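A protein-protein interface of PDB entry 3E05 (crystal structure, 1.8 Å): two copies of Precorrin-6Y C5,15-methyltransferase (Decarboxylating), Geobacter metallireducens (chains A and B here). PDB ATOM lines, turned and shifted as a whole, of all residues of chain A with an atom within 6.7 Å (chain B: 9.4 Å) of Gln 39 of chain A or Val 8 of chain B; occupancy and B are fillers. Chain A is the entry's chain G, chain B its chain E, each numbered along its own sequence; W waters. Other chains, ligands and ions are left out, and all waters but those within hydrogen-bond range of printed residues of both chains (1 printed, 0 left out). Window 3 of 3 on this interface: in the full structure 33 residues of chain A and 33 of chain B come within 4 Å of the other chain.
The backbone carbonyl oxygen of Leu 38 of chain A is in hydrogen-bond range of the backbone NH of Val 8 of chain B, at 2.8 Å.
The backbone carbonyl oxygen (O) of Val 8 of chain B lies within hydrogen-bond range of the side-chain amide nitrogen (ND2) of Asn 60 of chain B (2.8 Å).
NE2 of Gln 39 of chain A sits at hydrogen-bond distance from O of Arg 37 of chain A.
The backbone carbonyl oxygen (O) of Arg 37 of chain A is in hydrogen-bond range of the guanidinium group (NH2) of Arg 111 of chain A.
Arg 37 of chain A touches Pro 7 of chain B (C to CB, 3.7 Å).
Pro 7 of chain B touches Leu 38 of chain A (CA to O, 3.3 Å).
Gln 39 of chain A touches Val 8 of chain B (CA to CG2, 3.97 Å).
CG2 of Val 8 of chain B touches O of Leu 61 of chain A, 3.8 Å away.
Leu 61 of chain A touches Leu 61 of chain B (CD2 to CD2, 3.5 Å).
Of the printed residues of chain B, Leu 38 of chain A touches Pro 7 and Val 8.
Of chain B, only Val 8 (3.97 Å) comes within 4 Å of Gln 39 of chain A.
Of the printed residues of chain B, Leu 61 of chain A touches Val 8 (3.8 Å) and Leu 61 (3.5 Å).
Of chain A, only Leu 38, Gln 39 and Leu 61 come within 4 Å of Val 8 of chain B.
Leu 38 of chain B touches none of the printed residues of chain A.
Of the printed residues of chain A, Leu 61 of chain B touches Leu 61.
The nearest residue of chain B that does not touch Gln 39 of chain A is Pro 7 of chain B (4.1 Å).
The nearest residue of chain A that does not touch Val 8 of chain B is Asp 40 of chain A (4.7 Å).
Printed residues of chain B that touch a printed residue of chain A: Pro 7, Val 8 and Leu 61.
Hydrophobic or aromatic side chains of chain B that line the printed part of chain A: Pro 7, Val 8 and Leu 61.
Hydrophobic or aromatic side chains of chain A within 4 Å of the printed part of chain B: Leu 61.
Among the printed residues, 6 pairs touch across the chains.
Among the printed residues, no Asp or Glu carboxylate lies within 4 Å of a Lys or Arg side-chain nitrogen of the other chain.
Leu 61 of chain B touches its own counterpart, Leu 61 of chain A.
Positions printed for both chains: 38, 60, 61 and 62.
Water W1 bridges the backbone carbonyl oxygen of Ile 9 of chain B (2.6 Å) and the backbone NH of Leu 38 of chain A (2.9 Å).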
ATOM      1  N   LEU A  36       9.509  24.455  22.794  1.00  0.00           N
ATOM      2  CA  LEU A  36      10.053  24.642  24.143  1.00  0.00           C
ATOM      3  C   LEU A  36      11.579  24.668  24.189  1.00  0.00           C
ATOM      4  O   LEU A  36      12.137  25.083  25.197  1.00  0.00           O
ATOM      5  CB  LEU A  36       9.496  23.592  25.118  1.00  0.00           C
ATOM      6  CG  LEU A  36       8.097  23.924  25.672  1.00  0.00           C
ATOM      7  CD1 LEU A  36       7.384  22.707  26.229  1.00  0.00           C
ATOM      8  CD2 LEU A  36       8.125  25.073  26.705  1.00  0.00           C
ATOM      9  N   ARG A  37      12.233  24.218  23.111  1.00  0.00           N
ATOM     10  CA  ARG A  37      13.694  24.302  22.947  1.00  0.00           C
ATOM     11  C   ARG A  37      14.432  23.608  24.104  1.00  0.00           C
ATOM     12  O   ARG A  37      15.323  24.180  24.722  1.00  0.00           O
ATOM     13  CB  ARG A  37      14.112  25.769  22.837  1.00  0.00           C
ATOM     14  CG  ARG A  37      14.999  26.102  21.664  1.00  0.00           C
ATOM     15  CD  ARG A  37      14.529  27.406  21.052  1.00  0.00           C
ATOM     16  NE  ARG A  37      13.158  27.250  20.568  1.00  0.00           N
ATOM     17  CZ  ARG A  37      12.338  28.243  20.237  1.00  0.00           C
ATOM     18  NH1 ARG A  37      11.114  27.951  19.813  1.00  0.00           N
ATOM     19  NH2 ARG A  37      12.728  29.515  20.325  1.00  0.00           N
ATOM     20  N   LEU A  38      14.040  22.373  24.380  1.00  0.00           N
ATOM     21  CA  LEU A  38      14.525  21.661  25.552  1.00  0.00           C
ATOM     22  C   LEU A  38      15.938  21.105  25.356  1.00  0.00           C
ATOM     23  O   LEU A  38      16.313  20.691  24.263  1.00  0.00           O
ATOM     24  CB  LEU A  38      13.568  20.532  25.906  1.00  0.00           C
ATOM     25  CG  LEU A  38      12.115  20.971  26.108  1.00  0.00           C
ATOM     26  CD1 LEU A  38      11.215  19.771  26.365  1.00  0.00           C
ATOM     27  CD2 LEU A  38      12.033  21.943  27.253  1.00  0.00           C
ATOM     28  N   GLN A  39      16.706  21.120  26.434  1.00  0.00           N
ATOM     29  CA  GLN A  39      18.013  20.484  26.483  1.00  0.00           C
ATOM     30  C   GLN A  39      18.133  19.962  27.898  1.00  0.00           C
ATOM     31  O   GLN A  39      17.413  20.430  28.771  1.00  0.00           O
ATOM     32  CB  GLN A  39      19.135  21.467  26.117  1.00  0.00           C
ATOM     33  CG  GLN A  39      19.170  22.760  26.909  1.00  0.00           C
ATOM     34  CD  GLN A  39      19.323  23.986  26.015  1.00  0.00           C
ATOM     35  OE1 GLN A  39      20.229  24.803  26.198  1.00  0.00           O
ATOM     36  NE2 GLN A  39      18.428  24.117  25.038  1.00  0.00           N
ATOM     37  N   ASP A  40      19.011  18.992  28.130  1.00  0.00           N
ATOM     38  CA  ASP A  40      19.097  18.354  29.450  1.00  0.00           C
ATOM     39  C   ASP A  40      19.467  19.364  30.538  1.00  0.00           C
ATOM     40  O   ASP A  40      19.932  20.464  30.229  1.00  0.00           O
ATOM     41  CB  ASP A  40      20.077  17.174  29.429  1.00  0.00           C
ATOM     42  CG  ASP A  40      19.668  16.055  30.381  1.00  0.00           C
ATOM     43  OD1 ASP A  40      18.728  16.246  31.182  1.00  0.00           O
ATOM     44  OD2 ASP A  40      20.280  14.971  30.330  1.00  0.00           O
ATOM     45  N   ASP A  41      19.218  18.996  31.799  1.00  0.00           N
ATOM     46  CA  ASP A  41      19.570  19.818  32.986  1.00  0.00           C
ATOM     47  C   ASP A  41      18.749  21.107  33.201  1.00  0.00           C
ATOM     48  O   ASP A  41      19.044  21.887  34.113  1.00  0.00           O
ATOM     49  CB  ASP A  41      21.092  20.139  33.058  1.00  0.00           C
ATOM     50  CG  ASP A  41      21.980  18.937  32.720  1.00  0.00           C
ATOM     51  OD1 ASP A  41      21.775  17.847  33.301  1.00  0.00           O
ATOM     52  OD2 ASP A  41      22.891  19.092  31.870  1.00  0.00           O
ATOM     53  N   LEU A  42      17.709  21.334  32.397  1.00  0.00           N
ATOM     54  CA  LEU A  42      16.912  22.546  32.558  1.00  0.00           C
ATOM     55  C   LEU A  42      15.829  22.392  33.635  1.00  0.00           C
ATOM     56  O   LEU A  42      15.456  21.271  33.996  1.00  0.00           O
ATOM     57  CB  LEU A  42      16.265  22.958  31.230  1.00  0.00           C
ATOM     58  CG  LEU A  42      17.086  23.427  30.025  1.00  0.00           C
ATOM     59  CD1 LEU A  42      16.133  23.942  28.940  1.00  0.00           C
ATOM     60  CD2 LEU A  42      18.104  24.502  30.377  1.00  0.00           C
ATOM     61  N   VAL A  43      15.348  23.520  34.147  1.00  0.00           N
ATOM     62  CA  VAL A  43      14.145  23.548  34.997  1.00  0.00           C
ATOM     63  C   VAL A  43      12.953  24.009  34.145  1.00  0.00           C
ATOM     64  O   VAL A  43      12.991  25.084  33.568  1.00  0.00           O
ATOM     65  CB  VAL A  43      14.291  24.516  36.199  1.00  0.00           C
ATOM     66  CG1 VAL A  43      12.966  24.678  36.943  1.00  0.00           C
ATOM     67  CG2 VAL A  43      15.388  24.020  37.178  1.00  0.00           C
ATOM     68  N   ASN A  60      11.435  12.736  29.159  1.00  0.00           N
ATOM     69  CA  ASN A  60      12.232  11.906  28.255  1.00  0.00           C
ATOM     70  C   ASN A  60      13.319  12.685  27.523  1.00  0.00           C
ATOM     71  O   ASN A  60      14.386  12.137  27.217  1.00  0.00           O
ATOM     72  CB  ASN A  60      11.330  11.228  27.222  1.00  0.00           C
ATOM     73  CG  ASN A  60      10.369  10.232  27.833  1.00  0.00           C
ATOM     74  OD1 ASN A  60      10.489   9.838  29.000  1.00  0.00           O
ATOM     75  ND2 ASN A  60       9.410   9.801  27.037  1.00  0.00           N
ATOM     76  N   LEU A  61      13.048  13.958  27.233  1.00  0.00           N
ATOM     77  CA  LEU A  61      13.995  14.802  26.521  1.00  0.00           C
ATOM     78  C   LEU A  61      15.068  15.332  27.461  1.00  0.00           C
ATOM     79  O   LEU A  61      16.183  15.630  27.029  1.00  0.00           O
ATOM     80  CB  LEU A  61      13.285  15.968  25.806  1.00  0.00           C
ATOM     81  CG  LEU A  61      12.224  15.683  24.726  1.00  0.00           C
ATOM     82  CD1 LEU A  61      11.897  16.931  23.903  1.00  0.00           C
ATOM     83  CD2 LEU A  61      12.711  14.600  23.817  1.00  0.00           C
ATOM     84  N   MET A  62      14.720  15.490  28.736  1.00  0.00           N
ATOM     85  CA  MET A  62      15.677  15.970  29.744  1.00  0.00           C
ATOM     86  C   MET A  62      15.733  15.032  30.947  1.00  0.00           C
ATOM     87  O   MET A  62      15.139  15.330  31.989  1.00  0.00           O
ATOM     88  CB  MET A  62      15.328  17.382  30.238  1.00  0.00           C
ATOM     89  CG  MET A  62      14.977  18.411  29.183  1.00  0.00           C
ATOM     90  SD  MET A  62      14.514  19.973  29.950  1.00  0.00           S
ATOM     91  CE  MET A  62      13.028  19.508  30.805  1.00  0.00           C
ATOM     92  N   GLY A  65      17.040  16.797  33.747  1.00  0.00           N
ATOM     93  CA  GLY A  65      16.326  18.061  33.953  1.00  0.00           C
ATOM     94  C   GLY A  65      15.360  17.984  35.128  1.00  0.00           C
ATOM     95  O   GLY A  65      15.239  16.949  35.784  1.00  0.00           O
ATOM     96  N   ARG A 111      12.231  27.070  31.295  1.00  0.00           N
ATOM     97  CA  ARG A 111      11.135  26.855  30.327  1.00  0.00           C
ATOM     98  C   ARG A 111       9.800  26.844  31.058  1.00  0.00           C
ATOM     99  O   ARG A 111       9.694  26.242  32.113  1.00  0.00           O
ATOM    100  CB  ARG A 111      11.297  25.504  29.619  1.00  0.00           C
ATOM    101  CG  ARG A 111      12.571  25.317  28.788  1.00  0.00           C
ATOM    102  CD  ARG A 111      12.705  26.425  27.789  1.00  0.00           C
ATOM    103  NE  ARG A 111      13.870  26.254  26.921  1.00  0.00           N
ATOM    104  CZ  ARG A 111      15.012  26.917  27.073  1.00  0.00           C
ATOM    105  NH1 ARG A 111      15.146  27.804  28.054  1.00  0.00           N
ATOM    106  NH2 ARG A 111      16.013  26.704  26.229  1.00  0.00           N
ATOM    107  N   GLN B   5      24.048  24.243  23.642  1.00  0.00           N
ATOM    108  CA  GLN B   5      23.694  25.455  22.833  1.00  0.00           C
ATOM    109  C   GLN B   5      22.613  25.184  21.763  1.00  0.00           C
ATOM    110  O   GLN B   5      22.028  26.123  21.216  1.00  0.00           O
ATOM    111  CB  GLN B   5      24.955  26.082  22.209  1.00  0.00           C
ATOM    112  CG  GLN B   5      25.408  25.435  20.904  1.00  0.00           C
ATOM    113  CD  GLN B   5      26.913  25.422  20.719  1.00  0.00           C
ATOM    114  OE1 GLN B   5      27.623  24.684  21.400  1.00  0.00           O
ATOM    115  NE2 GLN B   5      27.402  26.216  19.771  1.00  0.00           N
ATOM    116  N   TYR B   6      22.369  23.905  21.469  1.00  0.00           N
ATOM    117  CA  TYR B   6      21.268  23.490  20.581  1.00  0.00           C
ATOM    118  C   TYR B   6      20.288  22.586  21.332  1.00  0.00           C
ATOM    119  O   TYR B   6      20.702  21.789  22.186  1.00  0.00           O
ATOM    120  CB  TYR B   6      21.789  22.792  19.316  1.00  0.00           C
ATOM    121  CG  TYR B   6      22.717  23.660  18.490  1.00  0.00           C
ATOM    122  CD1 TYR B   6      22.272  24.862  17.925  1.00  0.00           C
ATOM    123  CD2 TYR B   6      24.040  23.275  18.268  1.00  0.00           C
ATOM    124  CE1 TYR B   6      23.131  25.667  17.177  1.00  0.00           C
ATOM    125  CE2 TYR B   6      24.901  24.067  17.517  1.00  0.00           C
ATOM    126  CZ  TYR B   6      24.444  25.259  16.977  1.00  0.00           C
ATOM    127  OH  TYR B   6      25.305  26.032  16.234  1.00  0.00           O
ATOM    128  N   PRO B   7      18.978  22.724  21.042  1.00  0.00           N
ATOM    129  CA  PRO B   7      17.998  21.850  21.700  1.00  0.00           C
ATOM    130  C   PRO B   7      18.034  20.419  21.181  1.00  0.00           C
ATOM    131  O   PRO B   7      18.655  20.149  20.151  1.00  0.00           O
ATOM    132  CB  PRO B   7      16.656  22.528  21.386  1.00  0.00           C
ATOM    133  CG  PRO B   7      16.895  23.292  20.130  1.00  0.00           C
ATOM    134  CD  PRO B   7      18.341  23.718  20.152  1.00  0.00           C
ATOM    135  N   VAL B   8      17.400  19.509  21.916  1.00  0.00           N
ATOM    136  CA  VAL B   8      17.295  18.103  21.549  1.00  0.00           C
ATOM    137  C   VAL B   8      16.470  17.975  20.261  1.00  0.00           C
ATOM    138  O   VAL B   8      16.869  17.273  19.313  1.00  0.00           O
ATOM    139  CB  VAL B   8      16.684  17.268  22.718  1.00  0.00           C
ATOM    140  CG1 VAL B   8      16.575  15.789  22.354  1.00  0.00           C
ATOM    141  CG2 VAL B   8      17.533  17.441  23.984  1.00  0.00           C
ATOM    142  N   ILE B   9      15.326  18.658  20.229  1.00  0.00           N
ATOM    143  CA  ILE B   9      14.530  18.818  18.999  1.00  0.00           C
ATOM    144  C   ILE B   9      14.126  20.290  18.947  1.00  0.00           C
ATOM    145  O   ILE B   9      14.167  20.979  19.966  1.00  0.00           O
ATOM    146  CB  ILE B   9      13.282  17.855  18.925  1.00  0.00           C
ATOM    147  CG1 ILE B   9      12.240  18.215  19.994  1.00  0.00           C
ATOM    148  CG2 ILE B   9      13.706  16.360  18.976  1.00  0.00           C
ATOM    149  CD1 ILE B   9      10.862  17.543  19.837  1.00  0.00           C
ATOM    150  N   GLY B  10      13.738  20.784  17.777  1.00  0.00           N
ATOM    151  CA  GLY B  10      13.347  22.184  17.660  1.00  0.00           C
ATOM    152  C   GLY B  10      14.469  23.124  17.286  1.00  0.00           C
ATOM    153  O   GLY B  10      14.361  24.342  17.480  1.00  0.00           O
ATOM    154  N   ILE B  11      15.545  22.553  16.750  1.00  0.00           N
ATOM    155  CA  ILE B  11      16.662  23.340  16.211  1.00  0.00           C
ATOM    156  C   ILE B  11      16.110  24.194  15.079  1.00  0.00           C
ATOM    157  O   ILE B  11      15.377  23.695  14.220  1.00  0.00           O
ATOM    158  CB  ILE B  11      17.838  22.432  15.718  1.00  0.00           C
ATOM    159  CG1 ILE B  11      18.391  21.576  16.862  1.00  0.00           C
ATOM    160  CG2 ILE B  11      18.975  23.285  15.054  1.00  0.00           C
ATOM    161  CD1 ILE B  11      19.385  20.506  16.408  1.00  0.00           C
ATOM    162  N   ASP B  12      16.412  25.488  15.127  1.00  0.00           N
ATOM    163  CA  ASP B  12      15.941  26.448  14.140  1.00  0.00           C
ATOM    164  C   ASP B  12      16.340  26.045  12.716  1.00  0.00           C
ATOM    165  O   ASP B  12      17.474  25.624  12.489  1.00  0.00           O
ATOM    166  CB  ASP B  12      16.489  27.833  14.462  1.00  0.00           C
ATOM    167  CG  ASP B  12      15.645  28.940  13.866  1.00  0.00           C
ATOM    168  OD1 ASP B  12      14.934  29.618  14.645  1.00  0.00           O
ATOM    169  OD2 ASP B  12      15.680  29.121  12.627  1.00  0.00           O
ATOM    170  N   PHE B  16      20.583  24.887   9.887  1.00  0.00           N
ATOM    171  CA  PHE B  16      20.984  23.805   8.994  1.00  0.00           C
ATOM    172  C   PHE B  16      21.482  24.367   7.675  1.00  0.00           C
ATOM    173  O   PHE B  16      20.855  25.268   7.096  1.00  0.00           O
ATOM    174  CB  PHE B  16      19.814  22.842   8.738  1.00  0.00           C
ATOM    175  CG  PHE B  16      19.400  22.058   9.942  1.00  0.00           C
ATOM    176  CD1 PHE B  16      20.019  20.848  10.254  1.00  0.00           C
ATOM    177  CD2 PHE B  16      18.397  22.530  10.775  1.00  0.00           C
ATOM    178  CE1 PHE B  16      19.644  20.123  11.395  1.00  0.00           C
ATOM    179  CE2 PHE B  16      18.009  21.814  11.896  1.00  0.00           C
ATOM    180  CZ  PHE B  16      18.622  20.611  12.215  1.00  0.00           C
ATOM    181  N   ARG B  29       8.858  18.484  11.122  1.00  0.00           N
ATOM    182  CA  ARG B  29       9.984  17.636  11.573  1.00  0.00           C
ATOM    183  C   ARG B  29       9.672  17.011  12.923  1.00  0.00           C
ATOM    184  O   ARG B  29       9.846  15.814  13.103  1.00  0.00           O
ATOM    185  CB  ARG B  29      11.282  18.463  11.663  1.00  0.00           C
ATOM    186  CG  ARG B  29      12.572  17.627  11.866  1.00  0.00           C
ATOM    187  CD  ARG B  29      13.801  18.523  12.199  1.00  0.00           C
ATOM    188  NE  ARG B  29      13.922  19.659  11.308  1.00  0.00           N
ATOM    189  CZ  ARG B  29      14.056  20.926  11.675  1.00  0.00           C
ATOM    190  NH1 ARG B  29      14.143  21.291  12.956  1.00  0.00           N
ATOM    191  NH2 ARG B  29      14.139  21.841  10.732  1.00  0.00           N
ATOM    192  N   ALA B  30       9.191  17.834  13.861  1.00  0.00           N
ATOM    193  CA  ALA B  30       8.750  17.362  15.182  1.00  0.00           C
ATOM    194  C   ALA B  30       7.659  16.275  15.114  1.00  0.00           C
ATOM    195  O   ALA B  30       7.787  15.236  15.748  1.00  0.00           O
ATOM    196  CB  ALA B  30       8.292  18.532  16.035  1.00  0.00           C
ATOM    197  N   LEU B  33       9.164  13.037  13.628  1.00  0.00           N
ATOM    198  CA  LEU B  33       9.901  12.334  14.683  1.00  0.00           C
ATOM    199  C   LEU B  33       8.988  11.605  15.658  1.00  0.00           C
ATOM    200  O   LEU B  33       9.284  10.477  16.035  1.00  0.00           O
ATOM    201  CB  LEU B  33      10.798  13.299  15.447  1.00  0.00           C
ATOM    202  CG  LEU B  33      11.994  13.850  14.661  1.00  0.00           C
ATOM    203  CD1 LEU B  33      12.561  15.007  15.429  1.00  0.00           C
ATOM    204  CD2 LEU B  33      13.060  12.792  14.382  1.00  0.00           C
ATOM    205  N   LEU B  38      10.266   6.625  18.193  1.00  0.00           N
ATOM    206  CA  LEU B  38      11.669   6.370  18.450  1.00  0.00           C
ATOM    207  C   LEU B  38      11.872   5.937  19.898  1.00  0.00           C
ATOM    208  O   LEU B  38      11.286   6.502  20.819  1.00  0.00           O
ATOM    209  CB  LEU B  38      12.539   7.595  18.109  1.00  0.00           C
ATOM    210  CG  LEU B  38      12.524   8.091  16.649  1.00  0.00           C
ATOM    211  CD1 LEU B  38      13.441   9.283  16.458  1.00  0.00           C
ATOM    212  CD2 LEU B  38      12.863   6.996  15.629  1.00  0.00           C
ATOM    213  N   SER B  53      18.318  17.020   8.603  1.00  0.00           N
ATOM    214  CA  SER B  53      17.687  17.582   9.808  1.00  0.00           C
ATOM    215  C   SER B  53      16.873  16.555  10.573  1.00  0.00           C
ATOM    216  O   SER B  53      16.840  16.592  11.810  1.00  0.00           O
ATOM    217  CB  SER B  53      16.812  18.805   9.470  1.00  0.00           C
ATOM    218  OG  SER B  53      15.628  18.422   8.787  1.00  0.00           O
ATOM    219  N   VAL B  54      16.228  15.635   9.842  1.00  0.00           N
ATOM    220  CA  VAL B  54      15.476  14.543  10.465  1.00  0.00           C
ATOM    221  C   VAL B  54      16.418  13.551  11.146  1.00  0.00           C
ATOM    222  O   VAL B  54      16.166  13.145  12.259  1.00  0.00           O
ATOM    223  CB  VAL B  54      14.543  13.793   9.470  1.00  0.00           C
ATOM    224  CG1 VAL B  54      13.898  12.585  10.134  1.00  0.00           C
ATOM    225  CG2 VAL B  54      13.456  14.718   8.950  1.00  0.00           C
ATOM    226  N   SER B  55      17.496  13.170  10.456  1.00  0.00           N
ATOM    227  CA  SER B  55      18.531  12.274  10.997  1.00  0.00           C
ATOM    228  C   SER B  55      19.176  12.840  12.267  1.00  0.00           C
ATOM    229  O   SER B  55      19.418  12.116  13.224  1.00  0.00           O
ATOM    230  CB  SER B  55      19.611  12.044   9.941  1.00  0.00           C
ATOM    231  OG  SER B  55      19.274  10.948   9.110  1.00  0.00           O
ATOM    232  N   ILE B  56      19.424  14.142  12.258  1.00  0.00           N
ATOM    233  CA  ILE B  56      20.112  14.821  13.364  1.00  0.00           C
ATOM    234  C   ILE B  56      19.249  14.862  14.633  1.00  0.00           C
ATOM    235  O   ILE B  56      19.699  14.499  15.738  1.00  0.00           O
ATOM    236  CB  ILE B  56      20.621  16.217  12.911  1.00  0.00           C
ATOM    237  CG1 ILE B  56      21.849  16.030  12.009  1.00  0.00           C
ATOM    238  CG2 ILE B  56      20.927  17.149  14.110  1.00  0.00           C
ATOM    239  CD1 ILE B  56      22.116  17.157  11.084  1.00  0.00           C
ATOM    240  N   GLU B  57      17.995  15.263  14.477  1.00  0.00           N
ATOM    241  CA  GLU B  57      17.127  15.341  15.646  1.00  0.00           C
ATOM    242  C   GLU B  57      16.753  13.969  16.184  1.00  0.00           C
ATOM    243  O   GLU B  57      16.657  13.786  17.392  1.00  0.00           O
ATOM    244  CB  GLU B  57      15.947  16.261  15.368  1.00  0.00           C
ATOM    245  CG  GLU B  57      16.394  17.736  15.266  1.00  0.00           C
ATOM    246  CD  GLU B  57      15.238  18.738  15.380  1.00  0.00           C
ATOM    247  OE1 GLU B  57      14.065  18.306  15.529  1.00  0.00           O
ATOM    248  OE2 GLU B  57      15.495  19.957  15.318  1.00  0.00           O
ATOM    249  N   ALA B  58      16.597  12.999  15.277  1.00  0.00           N
ATOM    250  CA  ALA B  58      16.441  11.598  15.643  1.00  0.00           C
ATOM    251  C   ALA B  58      17.651  11.081  16.443  1.00  0.00           C
ATOM    252  O   ALA B  58      17.482  10.292  17.378  1.00  0.00           O
ATOM    253  CB  ALA B  58      16.257  10.762  14.413  1.00  0.00           C
ATOM    254  N   SER B  59      18.844  11.536  16.059  1.00  0.00           N
ATOM    255  CA  SER B  59      20.091  11.162  16.741  1.00  0.00           C
ATOM    256  C   SER B  59      20.146  11.649  18.177  1.00  0.00           C
ATOM    257  O   SER B  59      20.655  10.938  19.053  1.00  0.00           O
ATOM    258  CB  SER B  59      21.326  11.601  15.946  1.00  0.00           C
ATOM    259  OG  SER B  59      21.741  12.910  16.259  1.00  0.00           O
ATOM    260  N   ASN B  60      19.616  12.849  18.417  1.00  0.00           N
ATOM    261  CA  ASN B  60      19.436  13.361  19.776  1.00  0.00           C
ATOM    262  C   ASN B  60      18.441  12.536  20.581  1.00  0.00           C
ATOM    263  O   ASN B  60      18.609  12.359  21.784  1.00  0.00           O
ATOM    264  CB  ASN B  60      18.995  14.826  19.752  1.00  0.00           C
ATOM    265  CG  ASN B  60      19.990  15.730  19.052  1.00  0.00           C
ATOM    266  OD1 ASN B  60      21.155  15.366  18.864  1.00  0.00           O
ATOM    267  ND2 ASN B  60      19.546  16.918  18.663  1.00  0.00           N
ATOM    268  N   LEU B  61      17.408  12.026  19.910  1.00  0.00           N
ATOM    269  CA  LEU B  61      16.383  11.226  20.568  1.00  0.00           C
ATOM    270  C   LEU B  61      16.851   9.790  20.839  1.00  0.00           C
ATOM    271  O   LEU B  61      16.346   9.133  21.752  1.00  0.00           O
ATOM    272  CB  LEU B  61      15.093  11.223  19.731  1.00  0.00           C
ATOM    273  CG  LEU B  61      14.321  12.553  19.619  1.00  0.00           C
ATOM    274  CD1 LEU B  61      13.091  12.410  18.721  1.00  0.00           C
ATOM    275  CD2 LEU B  61      13.913  13.010  20.975  1.00  0.00           C
ATOM    276  N   MET B  62      17.787   9.301  20.020  1.00  0.00           N
ATOM    277  CA  MET B  62      18.389   7.975  20.196  1.00  0.00           C
ATOM    278  C   MET B  62      19.912   8.073  20.258  1.00  0.00           C
ATOM    279  O   MET B  62      20.580   7.773  19.259  1.00  0.00           O
ATOM    280  CB  MET B  62      18.035   7.042  19.037  1.00  0.00           C
ATOM    281  CG  MET B  62      16.580   6.958  18.686  1.00  0.00           C
ATOM    282  SD  MET B  62      16.307   5.636  17.532  1.00  0.00           S
ATOM    283  CE  MET B  62      17.068   6.337  16.073  1.00  0.00           C
ATOM    284  N   PRO B  63      20.470   8.480  21.417  1.00  0.00           N
ATOM    285  CA  PRO B  63      21.936   8.636  21.509  1.00  0.00           C
ATOM    286  C   PRO B  63      22.700   7.306  21.344  1.00  0.00           C
ATOM    287  O   PRO B  63      23.771   7.290  20.753  1.00  0.00           O
ATOM    288  CB  PRO B  63      22.146   9.232  22.903  1.00  0.00           C
ATOM    289  CG  PRO B  63      20.915   8.849  23.689  1.00  0.00           C
ATOM    290  CD  PRO B  63      19.792   8.802  22.689  1.00  0.00           C
ATOM    291  N   PHE B  87      26.466  19.793  14.489  1.00  0.00           N
ATOM    292  CA  PHE B  87      25.553  19.365  15.544  1.00  0.00           C
ATOM    293  C   PHE B  87      26.061  18.182  16.368  1.00  0.00           C
ATOM    294  O   PHE B  87      25.413  17.764  17.338  1.00  0.00           O
ATOM    295  CB  PHE B  87      24.154  19.124  14.956  1.00  0.00           C
ATOM    296  CG  PHE B  87      23.527  20.381  14.398  1.00  0.00           C
ATOM    297  CD1 PHE B  87      23.065  21.377  15.254  1.00  0.00           C
ATOM    298  CD2 PHE B  87      23.440  20.589  13.025  1.00  0.00           C
ATOM    299  CE1 PHE B  87      22.519  22.539  14.755  1.00  0.00           C
ATOM    300  CE2 PHE B  87      22.889  21.755  12.517  1.00  0.00           C
ATOM    301  CZ  PHE B  87      22.432  22.733  13.382  1.00  0.00           C
HETATM  302  O   HOH W   1      12.852  20.846  22.262  1.00  0.00           O
